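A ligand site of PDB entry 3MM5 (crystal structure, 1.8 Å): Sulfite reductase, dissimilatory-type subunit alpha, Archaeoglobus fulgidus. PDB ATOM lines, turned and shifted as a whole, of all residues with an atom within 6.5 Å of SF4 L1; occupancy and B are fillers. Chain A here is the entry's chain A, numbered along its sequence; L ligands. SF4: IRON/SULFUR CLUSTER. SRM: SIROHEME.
The side-chain sulfur (SG) of Cys 182 sits close to an oxygen (O4A) of SRM L2, at 3.4 Å. N of Gly 219 lies close to S3 of SF4 L1. N of Asp 223 lies close to S3 of SF4 L1. The side-chain sulfur of Cys 220 binds an iron atom (FE1) of SF4 L1 (2.2 Å). A sulfur (S4) of SF4 L1 lies close to the side-chain amide nitrogen of Asn 222 (3.5 Å). An iron atom (FE2) of SF4 L1 is bound by the side-chain sulfur (SG) of Cys 224 (2.2 Å). N of Cys 220 lies close to S3 of SF4 L1 (3.6 Å). A sulfur (S3) of SF4 L1 lies close to the backbone NH (N) of Cys 224 (3.4 Å). FE of SRM L2 is bound by SG of Cys 224 (2.5 Å). A sulfur (S2) of SF4 L1 sits close to the backbone NH (N) of Ala 185 (3.7 Å). FE4 of SF4 L1 is bound by SG of Cys 176. The side-chain sulfur (SG) of Cys 182 binds an iron atom (FE3) of SF4 L1, at 2.3 Å. N of Met 177 is in hydrogen-bond range of O3B of SRM L2 (2.9 Å). The side-chain carboxylate (OE1) of Glu 183 lies close to an oxygen (O4A) of SRM L2, 3.1 Å away.
N of Gly 219 sits close to SG of Cys 176. The side-chain sulfur of Cys 176 sits close to the backbone NH of Gly 178 (3.3 Å). O of Cys 176 is in hydrogen-bond range of OG1 of Thr 189, at 2.8 Å. N of Cys 176 is in hydrogen-bond range of O of Cys 217 (3.0 Å). N of Phe 184 sits close to SG of Cys 182, 3.4 Å away. The backbone NH (N) of Cys 186 lies within hydrogen-bond range of the backbone carbonyl oxygen (O) of Gly 219. The backbone carbonyl oxygen (O) of Phe 184 lies within hydrogen-bond range of the side-chain sulfur (SG) of Cys 186, 3.7 Å away. ND2 of Asn 222 is in hydrogen-bond range of OD1 of Asn 294, at 2.8 Å.
Met 177 touches SF4 L1 (CG to S1, 3.7 Å). CD2 of Phe 184 touches S4 of SF4 L1, 3.7 Å away. Hydrophobic or aromatic side chains that line SF4 L1: Met 177, Phe 184 and Ala 185. Of the 21 residues printed, 10 come within 4 Å of SF4 L1. Along chain A the residues within 4 Å of SF4 L1 span positions 176 to 224.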
ATOM      1  N   CYS A 176      -9.657  18.422  27.615  1.00  0.00           N
ATOM      2  CA  CYS A 176      -9.899  16.957  27.550  1.00  0.00           C
ATOM      3  C   CYS A 176     -10.637  16.527  28.817  1.00  0.00           C
ATOM      4  O   CYS A 176     -10.729  17.281  29.774  1.00  0.00           O
ATOM      5  CB  CYS A 176      -8.574  16.252  27.438  1.00  0.00           C
ATOM      6  SG  CYS A 176      -7.777  16.096  29.066  1.00  0.00           S
ATOM      7  N   MET A 177     -11.170  15.306  28.817  1.00  0.00           N
ATOM      8  CA  MET A 177     -11.992  14.814  29.926  1.00  0.00           C
ATOM      9  C   MET A 177     -11.272  14.913  31.256  1.00  0.00           C
ATOM     10  O   MET A 177     -11.896  15.046  32.302  1.00  0.00           O
ATOM     11  CB  MET A 177     -12.429  13.358  29.645  1.00  0.00           C
ATOM     12  CG  MET A 177     -11.294  12.329  29.654  1.00  0.00           C
ATOM     13  SD  MET A 177     -11.938  10.867  28.809  1.00  0.00           S
ATOM     14  CE  MET A 177     -10.614   9.695  29.179  1.00  0.00           C
ATOM     15  N   GLY A 178      -9.955  14.803  31.224  1.00  0.00           N
ATOM     16  CA  GLY A 178      -9.174  14.999  32.415  1.00  0.00           C
ATOM     17  C   GLY A 178      -9.620  14.088  33.565  1.00  0.00           C
ATOM     18  O   GLY A 178     -10.069  12.968  33.313  1.00  0.00           O
ATOM     19  N   PRO A 179      -9.568  14.596  34.805  1.00  0.00           N
ATOM     20  CA  PRO A 179      -9.821  13.756  35.978  1.00  0.00           C
ATOM     21  C   PRO A 179     -11.277  13.296  36.088  1.00  0.00           C
ATOM     22  O   PRO A 179     -11.560  12.447  36.909  1.00  0.00           O
ATOM     23  CB  PRO A 179      -9.418  14.629  37.153  1.00  0.00           C
ATOM     24  CG  PRO A 179      -9.665  16.055  36.649  1.00  0.00           C
ATOM     25  CD  PRO A 179      -9.287  16.012  35.178  1.00  0.00           C
ATOM     26  N   CYS A 182     -10.158  10.151  33.546  1.00  0.00           N
ATOM     27  CA  CYS A 182      -8.870   9.667  33.053  1.00  0.00           C
ATOM     28  C   CYS A 182      -7.889   9.584  34.198  1.00  0.00           C
ATOM     29  O   CYS A 182      -7.664  10.580  34.880  1.00  0.00           O
ATOM     30  CB  CYS A 182      -8.328  10.611  31.972  1.00  0.00           C
ATOM     31  SG  CYS A 182      -6.875   9.888  31.205  1.00  0.00           S
ATOM     32  N   GLU A 183      -7.278   8.412  34.410  1.00  0.00           N
ATOM     33  CA  GLU A 183      -6.373   8.260  35.512  1.00  0.00           C
ATOM     34  C   GLU A 183      -5.018   8.894  35.161  1.00  0.00           C
ATOM     35  O   GLU A 183      -4.118   8.935  36.015  1.00  0.00           O
ATOM     36  CB  GLU A 183      -6.245   6.772  35.931  1.00  0.00           C
ATOM     37  CG  GLU A 183      -5.514   5.853  34.936  1.00  0.00           C
ATOM     38  CD  GLU A 183      -6.338   5.313  33.718  1.00  0.00           C
ATOM     39  OE1 GLU A 183      -7.320   5.959  33.205  1.00  0.00           O
ATOM     40  OE2 GLU A 183      -5.904   4.250  33.201  1.00  0.00           O
ATOM     41  N   PHE A 184      -4.883   9.410  33.940  1.00  0.00           N
ATOM     42  CA  PHE A 184      -3.613  10.069  33.516  1.00  0.00           C
ATOM     43  C   PHE A 184      -3.536  11.551  33.879  1.00  0.00           C
ATOM     44  O   PHE A 184      -2.489  12.164  33.780  1.00  0.00           O
ATOM     45  CB  PHE A 184      -3.273   9.892  32.016  1.00  0.00           C
ATOM     46  CG  PHE A 184      -3.124   8.428  31.558  1.00  0.00           C
ATOM     47  CD1 PHE A 184      -3.021   7.394  32.475  1.00  0.00           C
ATOM     48  CD2 PHE A 184      -3.071   8.109  30.201  1.00  0.00           C
ATOM     49  CE1 PHE A 184      -2.866   6.061  32.046  1.00  0.00           C
ATOM     50  CE2 PHE A 184      -2.922   6.780  29.757  1.00  0.00           C
ATOM     51  CZ  PHE A 184      -2.818   5.760  30.677  1.00  0.00           C
ATOM     52  N   ALA A 185      -4.642  12.146  34.267  1.00  0.00           N
ATOM     53  CA  ALA A 185      -4.749  13.636  34.292  1.00  0.00           C
ATOM     54  C   ALA A 185      -3.856  14.233  35.351  1.00  0.00           C
ATOM     55  O   ALA A 185      -3.830  13.754  36.458  1.00  0.00           O
ATOM     56  CB  ALA A 185      -6.191  14.049  34.493  1.00  0.00           C
ATOM     57  N   CYS A 186      -3.064  15.224  34.967  1.00  0.00           N
ATOM     58  CA  CYS A 186      -2.087  15.867  35.839  1.00  0.00           C
ATOM     59  C   CYS A 186      -2.619  17.131  36.514  1.00  0.00           C
ATOM     60  O   CYS A 186      -2.005  17.625  37.432  1.00  0.00           O
ATOM     61  CB  CYS A 186      -0.845  16.207  35.051  1.00  0.00           C
ATOM     62  SG  CYS A 186       0.018  14.707  34.664  1.00  0.00           S
ATOM     63  N   THR A 189      -8.405  19.702  34.337  1.00  0.00           N
ATOM     64  CA  THR A 189      -8.522  20.321  33.014  1.00  0.00           C
ATOM     65  C   THR A 189      -9.867  21.057  32.980  1.00  0.00           C
ATOM     66  O   THR A 189      -9.949  22.236  32.588  1.00  0.00           O
ATOM     67  CB  THR A 189      -8.438  19.288  31.850  1.00  0.00           C
ATOM     68  OG1 THR A 189      -9.415  18.259  32.029  1.00  0.00           O
ATOM     69  CG2 THR A 189      -7.002  18.652  31.759  1.00  0.00           C
ATOM     70  N   CYS A 217      -6.768  22.941  26.978  1.00  0.00           N
ATOM     71  CA  CYS A 217      -6.249  22.332  28.197  1.00  0.00           C
ATOM     72  C   CYS A 217      -6.250  20.832  28.075  1.00  0.00           C
ATOM     73  O   CYS A 217      -7.295  20.198  28.089  1.00  0.00           O
ATOM     74  CB  CYS A 217      -7.077  22.741  29.426  1.00  0.00           C
ATOM     75  SG  CYS A 217      -7.399  24.541  29.610  1.00  0.00           S
ATOM     76  N   ALA A 218      -5.058  20.259  27.971  1.00  0.00           N
ATOM     77  CA  ALA A 218      -4.880  18.814  27.931  1.00  0.00           C
ATOM     78  C   ALA A 218      -4.293  18.358  29.255  1.00  0.00           C
ATOM     79  O   ALA A 218      -3.417  19.006  29.784  1.00  0.00           O
ATOM     80  CB  ALA A 218      -3.949  18.434  26.787  1.00  0.00           C
ATOM     81  N   GLY A 219      -4.797  17.230  29.744  1.00  0.00           N
ATOM     82  CA  GLY A 219      -4.495  16.794  31.120  1.00  0.00           C
ATOM     83  C   GLY A 219      -3.134  16.161  31.218  1.00  0.00           C
ATOM     84  O   GLY A 219      -2.580  16.088  32.340  1.00  0.00           O
ATOM     85  N   CYS A 220      -2.600  15.741  30.064  1.00  0.00           N
ATOM     86  CA  CYS A 220      -1.268  15.067  30.054  1.00  0.00           C
ATOM     87  C   CYS A 220      -0.735  15.153  28.637  1.00  0.00           C
ATOM     88  O   CYS A 220      -1.407  15.628  27.738  1.00  0.00           O
ATOM     89  CB  CYS A 220      -1.371  13.581  30.505  1.00  0.00           C
ATOM     90  SG  CYS A 220      -2.012  12.419  29.299  1.00  0.00           S
ATOM     91  N   PRO A 221       0.501  14.726  28.420  1.00  0.00           N
ATOM     92  CA  PRO A 221       1.090  14.965  27.119  1.00  0.00           C
ATOM     93  C   PRO A 221       0.486  14.197  25.955  1.00  0.00           C
ATOM     94  O   PRO A 221       0.909  14.445  24.833  1.00  0.00           O
ATOM     95  CB  PRO A 221       2.520  14.462  27.289  1.00  0.00           C
ATOM     96  CG  PRO A 221       2.801  14.697  28.776  1.00  0.00           C
ATOM     97  CD  PRO A 221       1.501  14.290  29.424  1.00  0.00           C
ATOM     98  N   ASN A 222      -0.408  13.233  26.191  1.00  0.00           N
ATOM     99  CA  ASN A 222      -1.076  12.605  25.057  1.00  0.00           C
ATOM    100  C   ASN A 222      -1.820  13.669  24.237  1.00  0.00           C
ATOM    101  O   ASN A 222      -2.068  13.480  23.064  1.00  0.00           O
ATOM    102  CB  ASN A 222      -2.017  11.483  25.513  1.00  0.00           C
ATOM    103  CG  ASN A 222      -1.294  10.212  25.865  1.00  0.00           C
ATOM    104  OD1 ASN A 222      -0.328   9.862  25.230  1.00  0.00           O
ATOM    105  ND2 ASN A 222      -1.755   9.544  26.927  1.00  0.00           N
ATOM    106  N   ASP A 223      -2.200  14.784  24.905  1.00  0.00           N
ATOM    107  CA  ASP A 223      -2.789  15.965  24.245  1.00  0.00           C
ATOM    108  C   ASP A 223      -4.063  15.625  23.469  1.00  0.00           C
ATOM    109  O   ASP A 223      -4.162  15.852  22.256  1.00  0.00           O
ATOM    110  CB  ASP A 223      -1.778  16.674  23.314  1.00  0.00           C
ATOM    111  CG  ASP A 223      -2.189  18.098  22.972  1.00  0.00           C
ATOM    112  OD1 ASP A 223      -3.266  18.566  23.478  1.00  0.00           O
ATOM    113  OD2 ASP A 223      -1.473  18.736  22.120  1.00  0.00           O
ATOM    114  N   CYS A 224      -5.058  15.097  24.199  1.00  0.00           N
ATOM    115  CA  CYS A 224      -6.221  14.494  23.594  1.00  0.00           C
ATOM    116  C   CYS A 224      -7.179  15.592  23.129  1.00  0.00           C
ATOM    117  O   CYS A 224      -8.293  15.300  22.650  1.00  0.00           O
ATOM    118  CB  CYS A 224      -6.896  13.581  24.644  1.00  0.00           C
ATOM    119  SG  CYS A 224      -5.862  12.178  24.975  1.00  0.00           S
ATOM    120  N   VAL A 225      -6.777  16.862  23.270  1.00  0.00           N
ATOM    121  CA  VAL A 225      -7.570  17.920  22.599  1.00  0.00           C
ATOM    122  C   VAL A 225      -6.778  18.616  21.502  1.00  0.00           C
ATOM    123  O   VAL A 225      -7.244  19.659  20.949  1.00  0.00           O
ATOM    124  CB  VAL A 225      -8.146  19.003  23.572  1.00  0.00           C
ATOM    125  CG1 VAL A 225      -9.452  18.473  24.258  1.00  0.00           C
ATOM    126  CG2 VAL A 225      -7.100  19.467  24.576  1.00  0.00           C
ATOM    127  N   MET A 290       4.614   9.681  27.713  1.00  0.00           N
ATOM    128  CA  MET A 290       3.443   8.858  28.125  1.00  0.00           C
ATOM    129  C   MET A 290       3.480   7.354  27.688  1.00  0.00           C
ATOM    130  O   MET A 290       2.702   6.546  28.214  1.00  0.00           O
ATOM    131  CB  MET A 290       2.079   9.515  27.789  1.00  0.00           C
ATOM    132  CG  MET A 290       1.832  10.828  28.583  1.00  0.00           C
ATOM    133  SD  MET A 290       1.572  10.538  30.347  1.00  0.00           S
ATOM    134  CE  MET A 290       0.258   9.345  30.362  1.00  0.00           C
ATOM    135  N   ASN A 294       0.861   4.594  29.006  1.00  0.00           N
ATOM    136  CA  ASN A 294      -0.223   4.224  28.067  1.00  0.00           C
ATOM    137  C   ASN A 294      -0.263   2.699  27.911  1.00  0.00           C
ATOM    138  O   ASN A 294      -1.333   2.110  27.818  1.00  0.00           O
ATOM    139  CB  ASN A 294      -0.005   4.856  26.671  1.00  0.00           C
ATOM    140  CG  ASN A 294      -0.056   6.389  26.656  1.00  0.00           C
ATOM    141  OD1 ASN A 294      -0.639   7.025  27.542  1.00  0.00           O
ATOM    142  ND2 ASN A 294       0.568   6.988  25.655  1.00  0.00           N
HETATM  143 FE1  SF4 L   1      -4.102  12.932  29.079  1.00  0.00          FE
HETATM  144 FE2  SF4 L   1      -5.879  12.347  27.178  1.00  0.00          FE
HETATM  145 FE3  SF4 L   1      -6.368  11.568  29.744  1.00  0.00          FE
HETATM  146 FE4  SF4 L   1      -6.493  14.189  29.047  1.00  0.00          FE
HETATM  147  S1  SF4 L   1      -7.866  12.427  28.308  1.00  0.00           S
HETATM  148  S2  SF4 L   1      -5.519  13.386  30.865  1.00  0.00           S
HETATM  149  S3  SF4 L   1      -4.772  14.398  27.497  1.00  0.00           S
HETATM  150  S4  SF4 L   1      -4.752  10.839  28.316  1.00  0.00           S
HETATM  151 FE   SRM L   2      -6.696  10.117  23.782  1.00  0.00          FE
HETATM  152  CHA SRM L   2      -5.128   7.420  25.306  1.00  0.00           C
HETATM  153  CHB SRM L   2      -9.408   9.471  25.616  1.00  0.00           C
HETATM  154  CHC SRM L   2      -8.563  12.120  21.690  1.00  0.00           C
HETATM  155  CHD SRM L   2      -4.070  10.531  21.703  1.00  0.00           C
HETATM  156  NA  SRM L   2      -7.149   8.823  25.243  1.00  0.00           N
HETATM  157  C1A SRM L   2      -6.390   7.840  25.772  1.00  0.00           C
HETATM  158  C2A SRM L   2      -6.998   7.122  26.970  1.00  0.00           C
HETATM  159  CMA SRM L   2      -6.755   5.573  26.935  1.00  0.00           C
HETATM  160  CDA SRM L   2      -6.516   7.688  28.333  1.00  0.00           C
HETATM  161  CEA SRM L   2      -6.973   6.917  29.554  1.00  0.00           C
HETATM  162  O3A SRM L   2      -8.167   6.562  29.619  1.00  0.00           O
HETATM  163  O4A SRM L   2      -6.142   6.666  30.465  1.00  0.00           O
HETATM  164  C3A SRM L   2      -8.456   7.450  26.789  1.00  0.00           C
HETATM  165  CAA SRM L   2      -9.203   6.296  26.001  1.00  0.00           C
HETATM  166  CBA SRM L   2      -8.866   6.198  24.469  1.00  0.00           C
HETATM  167  CCA SRM L   2      -9.039   4.809  23.874  1.00  0.00           C
HETATM  168  O1A SRM L   2      -9.908   4.617  22.995  1.00  0.00           O
HETATM  169  O2A SRM L   2      -8.285   3.870  24.249  1.00  0.00           O
HETATM  170  C4A SRM L   2      -8.308   8.621  25.815  1.00  0.00           C
HETATM  171  NB  SRM L   2      -8.573  10.678  23.740  1.00  0.00           N
HETATM  172  C1B SRM L   2      -9.511  10.386  24.600  1.00  0.00           C
HETATM  173  C2B SRM L   2     -10.834  11.141  24.405  1.00  0.00           C
HETATM  174  CMB SRM L   2     -12.110  10.424  24.870  1.00  0.00           C
HETATM  175  CDB SRM L   2     -10.591  12.478  25.189  1.00  0.00           C
HETATM  176  CEB SRM L   2     -11.743  13.483  25.246  1.00  0.00           C
HETATM  177  O3B SRM L   2     -11.737  14.369  26.127  1.00  0.00           O
HETATM  178  O4B SRM L   2     -12.683  13.368  24.429  1.00  0.00           O
HETATM  179  C3B SRM L   2     -10.544  11.376  22.989  1.00  0.00           C
HETATM  180  CAB SRM L   2     -11.388  10.568  21.973  1.00  0.00           C
HETATM  181  CBB SRM L   2     -11.360  10.901  20.445  1.00  0.00           C
HETATM  182  CCB SRM L   2     -12.213   9.829  19.801  1.00  0.00           C
HETATM  183  O1B SRM L   2     -13.475   9.800  19.911  1.00  0.00           O
HETATM  184  O2B SRM L   2     -11.588   8.974  19.160  1.00  0.00           O
HETATM  185  C4B SRM L   2      -9.129  11.444  22.750  1.00  0.00           C
HETATM  186  NC  SRM L   2      -6.362  11.135  22.106  1.00  0.00           N
HETATM  187  C1C SRM L   2      -7.216  11.950  21.493  1.00  0.00           C
HETATM  188  C2C SRM L   2      -6.566  12.757  20.370  1.00  0.00           C
HETATM  189  CDC SRM L   2      -6.916  14.173  19.915  1.00  0.00           C
HETATM  190  CEC SRM L   2      -7.265  14.078  18.422  1.00  0.00           C
HETATM  191  O3C SRM L   2      -7.132  13.030  17.763  1.00  0.00           O
HETATM  192  O4C SRM L   2      -7.686  15.119  17.848  1.00  0.00           O
HETATM  193  C3C SRM L   2      -5.173  12.244  20.347  1.00  0.00           C
HETATM  194  CAC SRM L   2      -3.965  13.006  19.846  1.00  0.00           C
HETATM  195  CBC SRM L   2      -3.891  12.309  18.478  1.00  0.00           C
HETATM  196  CCC SRM L   2      -2.498  12.327  17.867  1.00  0.00           C
HETATM  197  O1C SRM L   2      -2.290  12.696  16.682  1.00  0.00           O
HETATM  198  O2C SRM L   2      -1.580  11.930  18.567  1.00  0.00           O
HETATM  199  C4C SRM L   2      -5.208  11.252  21.483  1.00  0.00           C
HETATM  200  ND  SRM L   2      -4.943   9.297  23.597  1.00  0.00           N
HETATM  201  C1D SRM L   2      -3.964   9.593  22.687  1.00  0.00           C
HETATM  202  C2D SRM L   2      -2.645   8.841  22.904  1.00  0.00           C
HETATM  203  CAD SRM L   2      -1.492   8.530  21.898  1.00  0.00           C
HETATM  204  CBD SRM L   2      -1.530   7.325  20.958  1.00  0.00           C
HETATM  205  CCD SRM L   2      -0.205   7.190  20.243  1.00  0.00           C
HETATM  206  O1D SRM L   2       0.216   6.027  20.154  1.00  0.00           O
HETATM  207  O2D SRM L   2       0.412   8.218  19.784  1.00  0.00           O
HETATM  208  C3D SRM L   2      -3.072   7.886  23.963  1.00  0.00           C
HETATM  209  CDD SRM L   2      -2.323   6.617  24.401  1.00  0.00           C
HETATM  210  CED SRM L   2      -3.039   5.300  24.076  1.00  0.00           C
HETATM  211  O3D SRM L   2      -3.077   4.886  22.905  1.00  0.00           O
HETATM  212  O4D SRM L   2      -3.562   4.639  25.031  1.00  0.00           O
HETATM  213  C4D SRM L   2      -4.502   8.164  24.262  1.00  0.00           C
